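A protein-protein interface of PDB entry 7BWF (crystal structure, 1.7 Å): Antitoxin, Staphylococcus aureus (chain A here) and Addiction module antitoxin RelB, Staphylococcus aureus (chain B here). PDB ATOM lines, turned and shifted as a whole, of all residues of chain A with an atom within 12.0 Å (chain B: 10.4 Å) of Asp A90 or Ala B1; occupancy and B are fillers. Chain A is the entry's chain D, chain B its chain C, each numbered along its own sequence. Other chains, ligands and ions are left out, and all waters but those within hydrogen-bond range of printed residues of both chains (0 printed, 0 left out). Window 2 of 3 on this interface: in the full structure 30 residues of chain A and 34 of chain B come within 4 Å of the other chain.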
ATOM      1  N   THR A  86      -3.630   9.297  -1.357  1.00  0.00           N
ATOM      2  CA  THR A  86      -3.728   8.045  -0.619  1.00  0.00           C
ATOM      3  C   THR A  86      -4.845   7.194  -1.204  1.00  0.00           C
ATOM      4  O   THR A  86      -6.015   7.602  -1.211  1.00  0.00           O
ATOM      5  CB  THR A  86      -3.982   8.297   0.863  1.00  0.00           C
ATOM      6  OG1 THR A  86      -2.924   9.105   1.388  1.00  0.00           O
ATOM      7  CG2 THR A  86      -4.026   6.975   1.611  1.00  0.00           C
ATOM      8  N   LYS A  87      -4.475   6.012  -1.683  1.00  0.00           N
ATOM      9  CA  LYS A  87      -5.399   5.086  -2.312  1.00  0.00           C
ATOM     10  C   LYS A  87      -5.193   3.692  -1.738  1.00  0.00           C
ATOM     11  O   LYS A  87      -4.057   3.250  -1.546  1.00  0.00           O
ATOM     12  CB  LYS A  87      -5.187   5.040  -3.834  1.00  0.00           C
ATOM     13  CG  LYS A  87      -5.634   6.280  -4.600  1.00  0.00           C
ATOM     14  CD  LYS A  87      -7.083   6.704  -4.333  1.00  0.00           C
ATOM     15  CE  LYS A  87      -7.751   7.132  -5.642  1.00  0.00           C
ATOM     16  NZ  LYS A  87      -8.690   8.274  -5.468  1.00  0.00           N
ATOM     17  N   ASP A  88      -6.298   3.009  -1.458  1.00  0.00           N
ATOM     18  CA  ASP A  88      -6.267   1.564  -1.282  1.00  0.00           C
ATOM     19  C   ASP A  88      -6.153   0.903  -2.648  1.00  0.00           C
ATOM     20  O   ASP A  88      -6.943   1.197  -3.550  1.00  0.00           O
ATOM     21  CB  ASP A  88      -7.528   1.072  -0.575  1.00  0.00           C
ATOM     22  CG  ASP A  88      -7.460   1.261   0.929  1.00  0.00           C
ATOM     23  OD1 ASP A  88      -6.512   0.766   1.573  1.00  0.00           O
ATOM     24  OD2 ASP A  88      -8.370   1.911   1.474  1.00  0.00           O
ATOM     25  N   ILE A  89      -5.162   0.026  -2.808  1.00  0.00           N
ATOM     26  CA  ILE A  89      -5.024  -0.757  -4.029  1.00  0.00           C
ATOM     27  C   ILE A  89      -4.931  -2.240  -3.694  1.00  0.00           C
ATOM     28  O   ILE A  89      -4.341  -2.640  -2.685  1.00  0.00           O
ATOM     29  CB  ILE A  89      -3.798  -0.330  -4.873  1.00  0.00           C
ATOM     30  CG1 ILE A  89      -2.484  -0.793  -4.235  1.00  0.00           C
ATOM     31  CG2 ILE A  89      -3.809   1.177  -5.060  1.00  0.00           C
ATOM     32  CD1 ILE A  89      -1.233  -0.142  -4.847  1.00  0.00           C
ATOM     33  N   ASP A  90      -5.501  -3.056  -4.576  1.00  0.00           N
ATOM     34  CA  ASP A  90      -5.432  -4.506  -4.478  1.00  0.00           C
ATOM     35  C   ASP A  90      -4.314  -5.049  -5.357  1.00  0.00           C
ATOM     36  O   ASP A  90      -3.999  -4.495  -6.414  1.00  0.00           O
ATOM     37  CB  ASP A  90      -6.760  -5.153  -4.881  1.00  0.00           C
ATOM     38  CG  ASP A  90      -7.950  -4.506  -4.197  1.00  0.00           C
ATOM     39  OD1 ASP A  90      -8.315  -4.944  -3.083  1.00  0.00           O
ATOM     40  OD2 ASP A  90      -8.518  -3.556  -4.779  1.00  0.00           O
ATOM     41  N   VAL A  91      -3.725  -6.149  -4.904  1.00  0.00           N
ATOM     42  CA  VAL A  91      -2.571  -6.740  -5.556  1.00  0.00           C
ATOM     43  C   VAL A  91      -3.054  -7.777  -6.562  1.00  0.00           C
ATOM     44  O   VAL A  91      -4.196  -7.733  -7.018  1.00  0.00           O
ATOM     45  CB  VAL A  91      -1.612  -7.378  -4.536  1.00  0.00           C
ATOM     46  CG1 VAL A  91      -0.760  -8.430  -5.220  1.00  0.00           C
ATOM     47  CG2 VAL A  91      -0.742  -6.318  -3.882  1.00  0.00           C
ATOM     48  N   ALA B   1      -5.385  -8.554  -0.211  1.00  0.00           N
ATOM     49  CA  ALA B   1      -5.391  -7.709  -1.399  1.00  0.00           C
ATOM     50  C   ALA B   1      -5.149  -6.252  -1.039  1.00  0.00           C
ATOM     51  O   ALA B   1      -4.126  -5.667  -1.402  1.00  0.00           O
ATOM     52  CB  ALA B   1      -6.714  -7.846  -2.138  1.00  0.00           C
ATOM     53  N   ARG B   2      -6.121  -5.674  -0.340  1.00  0.00           N
ATOM     54  CA  ARG B   2      -6.068  -4.270   0.031  1.00  0.00           C
ATOM     55  C   ARG B   2      -4.727  -3.930   0.660  1.00  0.00           C
ATOM     56  O   ARG B   2      -4.256  -4.618   1.573  1.00  0.00           O
ATOM     57  CB  ARG B   2      -7.210  -3.959   0.999  1.00  0.00           C
ATOM     58  CG  ARG B   2      -7.426  -2.494   1.321  1.00  0.00           C
ATOM     59  CD  ARG B   2      -8.390  -2.345   2.502  1.00  0.00           C
ATOM     60  NE  ARG B   2      -7.725  -2.599   3.779  1.00  0.00           N
ATOM     61  CZ  ARG B   2      -7.149  -1.655   4.520  1.00  0.00           C
ATOM     62  NH1 ARG B   2      -7.158  -0.391   4.114  1.00  0.00           N
ATOM     63  NH2 ARG B   2      -6.562  -1.972   5.666  1.00  0.00           N
ATOM     64  N   LEU B   3      -4.112  -2.872   0.134  1.00  0.00           N
ATOM     65  CA  LEU B   3      -2.881  -2.306   0.671  1.00  0.00           C
ATOM     66  C   LEU B   3      -2.956  -0.795   0.520  1.00  0.00           C
ATOM     67  O   LEU B   3      -3.056  -0.291  -0.603  1.00  0.00           O
ATOM     68  CB  LEU B   3      -1.653  -2.855  -0.058  1.00  0.00           C
ATOM     69  CG  LEU B   3      -0.282  -2.634   0.585  1.00  0.00           C
ATOM     70  CD1 LEU B   3      -0.182  -3.352   1.928  1.00  0.00           C
ATOM     71  CD2 LEU B   3       0.818  -3.106  -0.367  1.00  0.00           C
ATOM     72  N   ASN B   4      -2.920  -0.078   1.642  1.00  0.00           N
ATOM     73  CA  ASN B   4      -2.995   1.379   1.630  1.00  0.00           C
ATOM     74  C   ASN B   4      -1.632   1.950   1.255  1.00  0.00           C
ATOM     75  O   ASN B   4      -0.627   1.665   1.917  1.00  0.00           O
ATOM     76  CB  ASN B   4      -3.457   1.903   2.988  1.00  0.00           C
ATOM     77  CG  ASN B   4      -4.100   3.277   2.893  1.00  0.00           C
ATOM     78  OD1 ASN B   4      -3.560   4.266   3.394  1.00  0.00           O
ATOM     79  ND2 ASN B   4      -5.245   3.350   2.218  1.00  0.00           N
ATOM     80  N   ILE B   5      -1.607   2.734   0.178  1.00  0.00           N
ATOM     81  CA  ILE B   5      -0.381   3.262  -0.404  1.00  0.00           C
ATOM     82  C   ILE B   5      -0.517   4.771  -0.531  1.00  0.00           C
ATOM     83  O   ILE B   5      -1.562   5.274  -0.962  1.00  0.00           O
ATOM     84  CB  ILE B   5      -0.108   2.639  -1.788  1.00  0.00           C
ATOM     85  CG1 ILE B   5       0.150   1.131  -1.674  1.00  0.00           C
ATOM     86  CG2 ILE B   5       1.053   3.341  -2.458  1.00  0.00           C
ATOM     87  CD1 ILE B   5       1.256   0.737  -0.702  1.00  0.00           C
ATOM     88  N   PHE B   7       0.863   7.858  -2.610  1.00  0.00           N
ATOM     89  CA  PHE B   7       1.571   8.285  -3.814  1.00  0.00           C
ATOM     90  C   PHE B   7       1.931   9.770  -3.749  1.00  0.00           C
ATOM     91  O   PHE B   7       1.238  10.562  -3.110  1.00  0.00           O
ATOM     92  CB  PHE B   7       0.730   8.087  -5.092  1.00  0.00           C
ATOM     93  CG  PHE B   7       0.378   6.673  -5.402  1.00  0.00           C
ATOM     94  CD1 PHE B   7      -0.675   6.071  -4.749  1.00  0.00           C
ATOM     95  CD2 PHE B   7       1.058   5.958  -6.380  1.00  0.00           C
ATOM     96  CE1 PHE B   7      -1.032   4.765  -5.029  1.00  0.00           C
ATOM     97  CE2 PHE B   7       0.694   4.640  -6.672  1.00  0.00           C
ATOM     98  CZ  PHE B   7      -0.348   4.048  -5.984  1.00  0.00           C
ATOM     99  N   TYR B  15       1.165   5.904 -12.232  1.00  0.00           N
ATOM    100  CA  TYR B  15       0.485   4.663 -11.870  1.00  0.00           C
ATOM    101  C   TYR B  15      -0.836   4.538 -12.623  1.00  0.00           C
ATOM    102  O   TYR B  15      -1.127   3.493 -13.215  1.00  0.00           O
ATOM    103  CB  TYR B  15       0.260   4.606 -10.354  1.00  0.00           C
ATOM    104  CG  TYR B  15      -0.250   3.262  -9.876  1.00  0.00           C
ATOM    105  CD1 TYR B  15       0.612   2.187  -9.716  1.00  0.00           C
ATOM    106  CD2 TYR B  15      -1.592   3.069  -9.590  1.00  0.00           C
ATOM    107  CE1 TYR B  15       0.149   0.956  -9.281  1.00  0.00           C
ATOM    108  CE2 TYR B  15      -2.063   1.844  -9.152  1.00  0.00           C
ATOM    109  CZ  TYR B  15      -1.189   0.788  -8.995  1.00  0.00           C
ATOM    110  OH  TYR B  15      -1.651  -0.439  -8.560  1.00  0.00           O
ATOM    111  N   GLN B  19      -2.115   1.894 -15.484  1.00  0.00           N
ATOM    112  CA  GLN B  19      -3.342   1.130 -15.273  1.00  0.00           C
ATOM    113  C   GLN B  19      -4.136   1.000 -16.567  1.00  0.00           C
ATOM    114  O   GLN B  19      -4.676  -0.068 -16.871  1.00  0.00           O
ATOM    115  CB  GLN B  19      -4.212   1.787 -14.187  1.00  0.00           C
ATOM    116  CG  GLN B  19      -3.691   1.661 -12.768  1.00  0.00           C
ATOM    117  CD  GLN B  19      -4.793   1.795 -11.721  1.00  0.00           C
ATOM    118  OE1 GLN B  19      -5.319   0.798 -11.220  1.00  0.00           O
ATOM    119  NE2 GLN B  19      -5.166   3.032 -11.411  1.00  0.00           N
ATOM    120  N   LYS B  23      -0.702  -2.903 -18.382  1.00  0.00           N
ATOM    121  CA  LYS B  23      -1.071  -3.734 -17.240  1.00  0.00           C
ATOM    122  C   LYS B  23       0.045  -4.703 -16.872  1.00  0.00           C
ATOM    123  O   LYS B  23       0.131  -5.145 -15.722  1.00  0.00           O
ATOM    124  CB  LYS B  23      -2.395  -4.435 -17.564  1.00  0.00           C
ATOM    125  CG  LYS B  23      -3.519  -3.365 -17.656  1.00  0.00           C
ATOM    126  CD  LYS B  23      -4.857  -3.765 -18.307  1.00  0.00           C
ATOM    127  CE  LYS B  23      -5.595  -2.483 -18.808  1.00  0.00           C
ATOM    128  NZ  LYS B  23      -7.069  -2.416 -18.515  1.00  0.00           N
ATOM    129  N   VAL B  26       1.743  -2.422 -14.197  1.00  0.00           N
ATOM    130  CA  VAL B  26       1.019  -2.292 -12.938  1.00  0.00           C
ATOM    131  C   VAL B  26       1.128  -3.582 -12.135  1.00  0.00           C
ATOM    132  O   VAL B  26       1.265  -3.559 -10.906  1.00  0.00           O
ATOM    133  CB  VAL B  26      -0.446  -1.904 -13.208  1.00  0.00           C
ATOM    134  CG1 VAL B  26      -1.212  -1.925 -11.903  1.00  0.00           C
ATOM    135  CG2 VAL B  26      -0.510  -0.541 -13.866  1.00  0.00           C
ATOM    136  N   LYS B  27       1.072  -4.729 -12.813  1.00  0.00           N
ATOM    137  CA  LYS B  27       1.229  -5.998 -12.112  1.00  0.00           C
ATOM    138  C   LYS B  27       2.595  -6.072 -11.442  1.00  0.00           C
ATOM    139  O   LYS B  27       2.707  -6.477 -10.282  1.00  0.00           O
ATOM    140  CB  LYS B  27       1.042  -7.179 -13.076  1.00  0.00           C
ATOM    141  CG  LYS B  27       1.276  -8.541 -12.399  1.00  0.00           C
ATOM    142  CD  LYS B  27       1.715  -9.614 -13.400  1.00  0.00           C
ATOM    143  CE  LYS B  27       1.553 -11.027 -12.818  1.00  0.00           C
ATOM    144  NZ  LYS B  27       2.782 -11.544 -12.148  1.00  0.00           N
ATOM    145  N   LYS B  28       3.649  -5.688 -12.162  1.00  0.00           N
ATOM    146  CA  LYS B  28       4.986  -5.713 -11.580  1.00  0.00           C
ATOM    147  C   LYS B  28       5.074  -4.769 -10.387  1.00  0.00           C
ATOM    148  O   LYS B  28       5.564  -5.145  -9.318  1.00  0.00           O
ATOM    149  CB  LYS B  28       6.028  -5.347 -12.642  1.00  0.00           C
ATOM    150  CG  LYS B  28       7.477  -5.564 -12.201  1.00  0.00           C
ATOM    151  CD  LYS B  28       7.691  -6.914 -11.525  1.00  0.00           C
ATOM    152  CE  LYS B  28       9.137  -7.080 -11.057  1.00  0.00           C
ATOM    153  NZ  LYS B  28      10.103  -7.180 -12.185  1.00  0.00           N
ATOM    154  N   ILE B  29       4.596  -3.532 -10.552  1.00  0.00           N
ATOM    155  CA  ILE B  29       4.616  -2.568  -9.455  1.00  0.00           C
ATOM    156  C   ILE B  29       3.880  -3.130  -8.242  1.00  0.00           C
ATOM    157  O   ILE B  29       4.353  -3.021  -7.104  1.00  0.00           O
ATOM    158  CB  ILE B  29       4.014  -1.224  -9.908  1.00  0.00           C
ATOM    159  CG1 ILE B  29       4.930  -0.530 -10.923  1.00  0.00           C
ATOM    160  CG2 ILE B  29       3.781  -0.324  -8.699  1.00  0.00           C
ATOM    161  CD1 ILE B  29       4.228   0.530 -11.766  1.00  0.00           C
ATOM    162  N   ASN B  30       2.707  -3.729  -8.463  1.00  0.00           N
ATOM    163  CA  ASN B  30       1.926  -4.265  -7.353  1.00  0.00           C
ATOM    164  C   ASN B  30       2.678  -5.388  -6.653  1.00  0.00           C
ATOM    165  O   ASN B  30       2.643  -5.494  -5.424  1.00  0.00           O
ATOM    166  CB  ASN B  30       0.563  -4.752  -7.855  1.00  0.00           C
ATOM    167  CG  ASN B  30      -0.380  -3.610  -8.172  1.00  0.00           C
ATOM    168  OD1 ASN B  30      -0.107  -2.454  -7.839  1.00  0.00           O
ATOM    169  ND2 ASN B  30      -1.494  -3.922  -8.819  1.00  0.00           N
ATOM    170  N   GLU B  31       3.383  -6.224  -7.417  1.00  0.00           N
ATOM    171  CA  GLU B  31       4.168  -7.291  -6.805  1.00  0.00           C
ATOM    172  C   GLU B  31       5.319  -6.720  -5.981  1.00  0.00           C
ATOM    173  O   GLU B  31       5.627  -7.226  -4.899  1.00  0.00           O
ATOM    174  CB  GLU B  31       4.705  -8.242  -7.876  1.00  0.00           C
ATOM    175  CG  GLU B  31       3.656  -9.137  -8.507  1.00  0.00           C
ATOM    176  CD  GLU B  31       4.247  -9.979  -9.619  1.00  0.00           C
ATOM    177  OE1 GLU B  31       3.830 -11.142  -9.790  1.00  0.00           O
ATOM    178  OE2 GLU B  31       5.155  -9.475 -10.313  1.00  0.00           O
ATOM    179  N   LEU B  32       5.965  -5.664  -6.478  1.00  0.00           N
ATOM    180  CA  LEU B  32       7.011  -5.003  -5.704  1.00  0.00           C
ATOM    181  C   LEU B  32       6.445  -4.436  -4.408  1.00  0.00           C
ATOM    182  O   LEU B  32       7.061  -4.553  -3.346  1.00  0.00           O
ATOM    183  CB  LEU B  32       7.657  -3.895  -6.541  1.00  0.00           C
ATOM    184  CG  LEU B  32       8.459  -4.367  -7.755  1.00  0.00           C
ATOM    185  CD1 LEU B  32       8.914  -3.170  -8.584  1.00  0.00           C
ATOM    186  CD2 LEU B  32       9.645  -5.219  -7.325  1.00  0.00           C
ATOM    187  N   LEU B  33       5.261  -3.826  -4.472  1.00  0.00           N
ATOM    188  CA  LEU B  33       4.649  -3.263  -3.272  1.00  0.00           C
ATOM    189  C   LEU B  33       4.312  -4.360  -2.269  1.00  0.00           C
ATOM    190  O   LEU B  33       4.552  -4.208  -1.069  1.00  0.00           O
ATOM    191  CB  LEU B  33       3.394  -2.471  -3.649  1.00  0.00           C
ATOM    192  CG  LEU B  33       3.609  -1.201  -4.469  1.00  0.00           C
ATOM    193  CD1 LEU B  33       2.266  -0.664  -4.936  1.00  0.00           C
ATOM    194  CD2 LEU B  33       4.362  -0.172  -3.646  1.00  0.00           C
ATOM    195  N   LYS B  34       3.766  -5.481  -2.740  1.00  0.00           N
ATOM    196  CA  LYS B  34       3.505  -6.598  -1.834  1.00  0.00           C
ATOM    197  C   LYS B  34       4.801  -7.080  -1.187  1.00  0.00           C
ATOM    198  O   LYS B  34       4.836  -7.376   0.012  1.00  0.00           O
ATOM    199  CB  LYS B  34       2.819  -7.748  -2.582  1.00  0.00           C
ATOM    200  CG  LYS B  34       2.186  -8.770  -1.641  1.00  0.00           C
ATOM    201  CD  LYS B  34       1.294  -9.782  -2.361  1.00  0.00           C
ATOM    202  CE  LYS B  34       1.943 -10.368  -3.598  1.00  0.00           C
ATOM    203  NZ  LYS B  34       1.062 -11.393  -4.229  1.00  0.00           N
ATOM    204  N   SER B  35       5.887  -7.147  -1.962  1.00  0.00           N
ATOM    205  CA  SER B  35       7.158  -7.619  -1.415  1.00  0.00           C
ATOM    206  C   SER B  35       7.696  -6.653  -0.365  1.00  0.00           C
ATOM    207  O   SER B  35       8.230  -7.078   0.666  1.00  0.00           O
ATOM    208  CB  SER B  35       8.180  -7.812  -2.545  1.00  0.00           C
ATOM    209  OG  SER B  35       9.438  -8.230  -2.029  1.00  0.00           O
ATOM    210  N   ASP B  37       5.864  -4.714   1.521  1.00  0.00           N
ATOM    211  CA  ASP B  37       4.987  -4.895   2.672  1.00  0.00           C
ATOM    212  C   ASP B  37       5.408  -6.104   3.497  1.00  0.00           C
ATOM    213  O   ASP B  37       5.534  -6.025   4.722  1.00  0.00           O
ATOM    214  CB  ASP B  37       3.548  -5.051   2.181  1.00  0.00           C
ATOM    215  CG  ASP B  37       2.545  -5.102   3.312  1.00  0.00           C
ATOM    216  OD1 ASP B  37       2.649  -4.281   4.248  1.00  0.00           O
ATOM    217  OD2 ASP B  37       1.644  -5.953   3.252  1.00  0.00           O
ATOM    218  N   ARG B  38       5.665  -7.231   2.839  1.00  0.00           N
ATOM    219  CA  ARG B  38       5.926  -8.462   3.577  1.00  0.00           C
ATOM    220  C   ARG B  38       7.347  -8.492   4.119  1.00  0.00           C
ATOM    221  O   ARG B  38       7.577  -8.878   5.271  1.00  0.00           O
ATOM    222  CB  ARG B  38       5.702  -9.686   2.686  1.00  0.00           C
ATOM    223  CG  ARG B  38       4.326 -10.248   2.760  1.00  0.00           C
ATOM    224  CD  ARG B  38       4.085 -11.145   1.568  1.00  0.00           C
ATOM    225  NE  ARG B  38       2.667 -11.402   1.389  1.00  0.00           N
ATOM    226  CZ  ARG B  38       2.149 -12.202   0.463  1.00  0.00           C
ATOM    227  NH1 ARG B  38       0.833 -12.357   0.405  1.00  0.00           N
ATOM    228  NH2 ARG B  38       2.928 -12.845  -0.399  1.00  0.00           N
ATOM    229  N   ILE B  78       3.889   2.380   3.222  1.00  0.00           N
ATOM    230  CA  ILE B  78       4.710   2.560   2.036  1.00  0.00           C
ATOM    231  C   ILE B  78       4.327   3.862   1.354  1.00  0.00           C
ATOM    232  O   ILE B  78       3.140   4.151   1.156  1.00  0.00           O
ATOM    233  CB  ILE B  78       4.548   1.378   1.070  1.00  0.00           C
ATOM    234  CG1 ILE B  78       5.048   0.076   1.696  1.00  0.00           C
ATOM    235  CG2 ILE B  78       5.296   1.667  -0.209  1.00  0.00           C
ATOM    236  CD1 ILE B  78       4.596  -1.178   0.938  1.00  0.00           C
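The backbone carbonyl oxygen (O) of Val B26 lies close to the side-chain amide nitrogen (ND2) of Asn B30 (3.5 Å). OD1 of Asn B30 is in hydrogen-bond range of OH of Tyr B15 (2.6 Å).
Of the printed residues of chain B, Asp A90 touches Ala B1, Arg B2 and Asn B30. Ala B1 touches just these residues of chain A: Ile A89 (3.3 Å), Asp A90 (3.4 Å) and Val A91 (3.6 Å). Ile A89 touches just these residues of chain B: Ala B1, Arg B2, Leu B3, Ile B5, Tyr B15, Asn B30 and Leu B33. Of chain B, only Ala B1 (3.6 Å), Asn B30 (3.8 Å) and Lys B34 (3.6 Å) come within 4 Å of Val A91. Leu B3 touches just these residues of chain A: Lys A87, Asp A88 and Ile A89. Printed residues of chain A within 4 Å of Leu B33: Ile A89 (3.5 Å). Of the printed residues of chain B, Asp A88 touches Arg B2 (2.9 Å), Leu B3 (3.8 Å) and Asn B4 (2.9 Å). Ile B78 touches none of the printed residues of chain A. The nearest residue of chain B that does not touch Asp A90 is Leu B3 (4.9 Å). The nearest printed residue of chain B that does not touch Asp A88 is Ile B5 (5.0 Å).
Among the printed residues, pairs that only touch across the chains: Thr A86 with Asn B4, Thr A86 with Ile B5, Lys A87 with Leu B3, Lys A87 with Asn B4, Asp A88 with Leu B3, Ile A89 with Arg B2, Ile A89 with Ile B5, Ile A89 with Tyr B15, Ile A89 with Asn B30, Ile A89 with Leu B33, Asp A90 with Ala B1, Asp A90 with Arg B2, Asp A90 with Asn B30, Val A91 with Ala B1, Val A91 with Asn B30 and Val A91 with Lys B34.
Printed residues of chain B that touch a printed residue of chain A: Ala B1, Arg B2, Leu B3, Asn B4, Ile B5, Tyr B15, Asn B30, Leu B33 and Lys B34. Hydrophobic or aromatic side chains of chain B within 4 Å of the printed part of chain A: Ala B1, Leu B3, Ile B5, Tyr B15 and Leu B33. Along chain B the printed residues that touch a printed residue of chain A span positions 1 to 34. Hydrophobic or aromatic side chains of chain A within 4 Å of the printed part of chain B: Ile A89 and Val A91. Among the printed residues, 21 pairs touch across the chains.
NH1 of Arg B2 lies within salt-bridge range of OD1 of Asp A88 (2.9 Å). O of Ile A89 lies close to O of Ala B1, 3.3 Å away. N of Leu B3 sits at hydrogen-bond distance from O of Ile A89, at 2.8 Å. The side-chain amide nitrogen (ND2) of Asn B4 sits at hydrogen-bond distance from the side-chain carboxylate (OD1) of Asp A88, 2.9 Å away. The backbone carbonyl oxygen of Lys A87 sits at hydrogen-bond distance from the backbone NH of Ile B5, 3.0 Å away.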
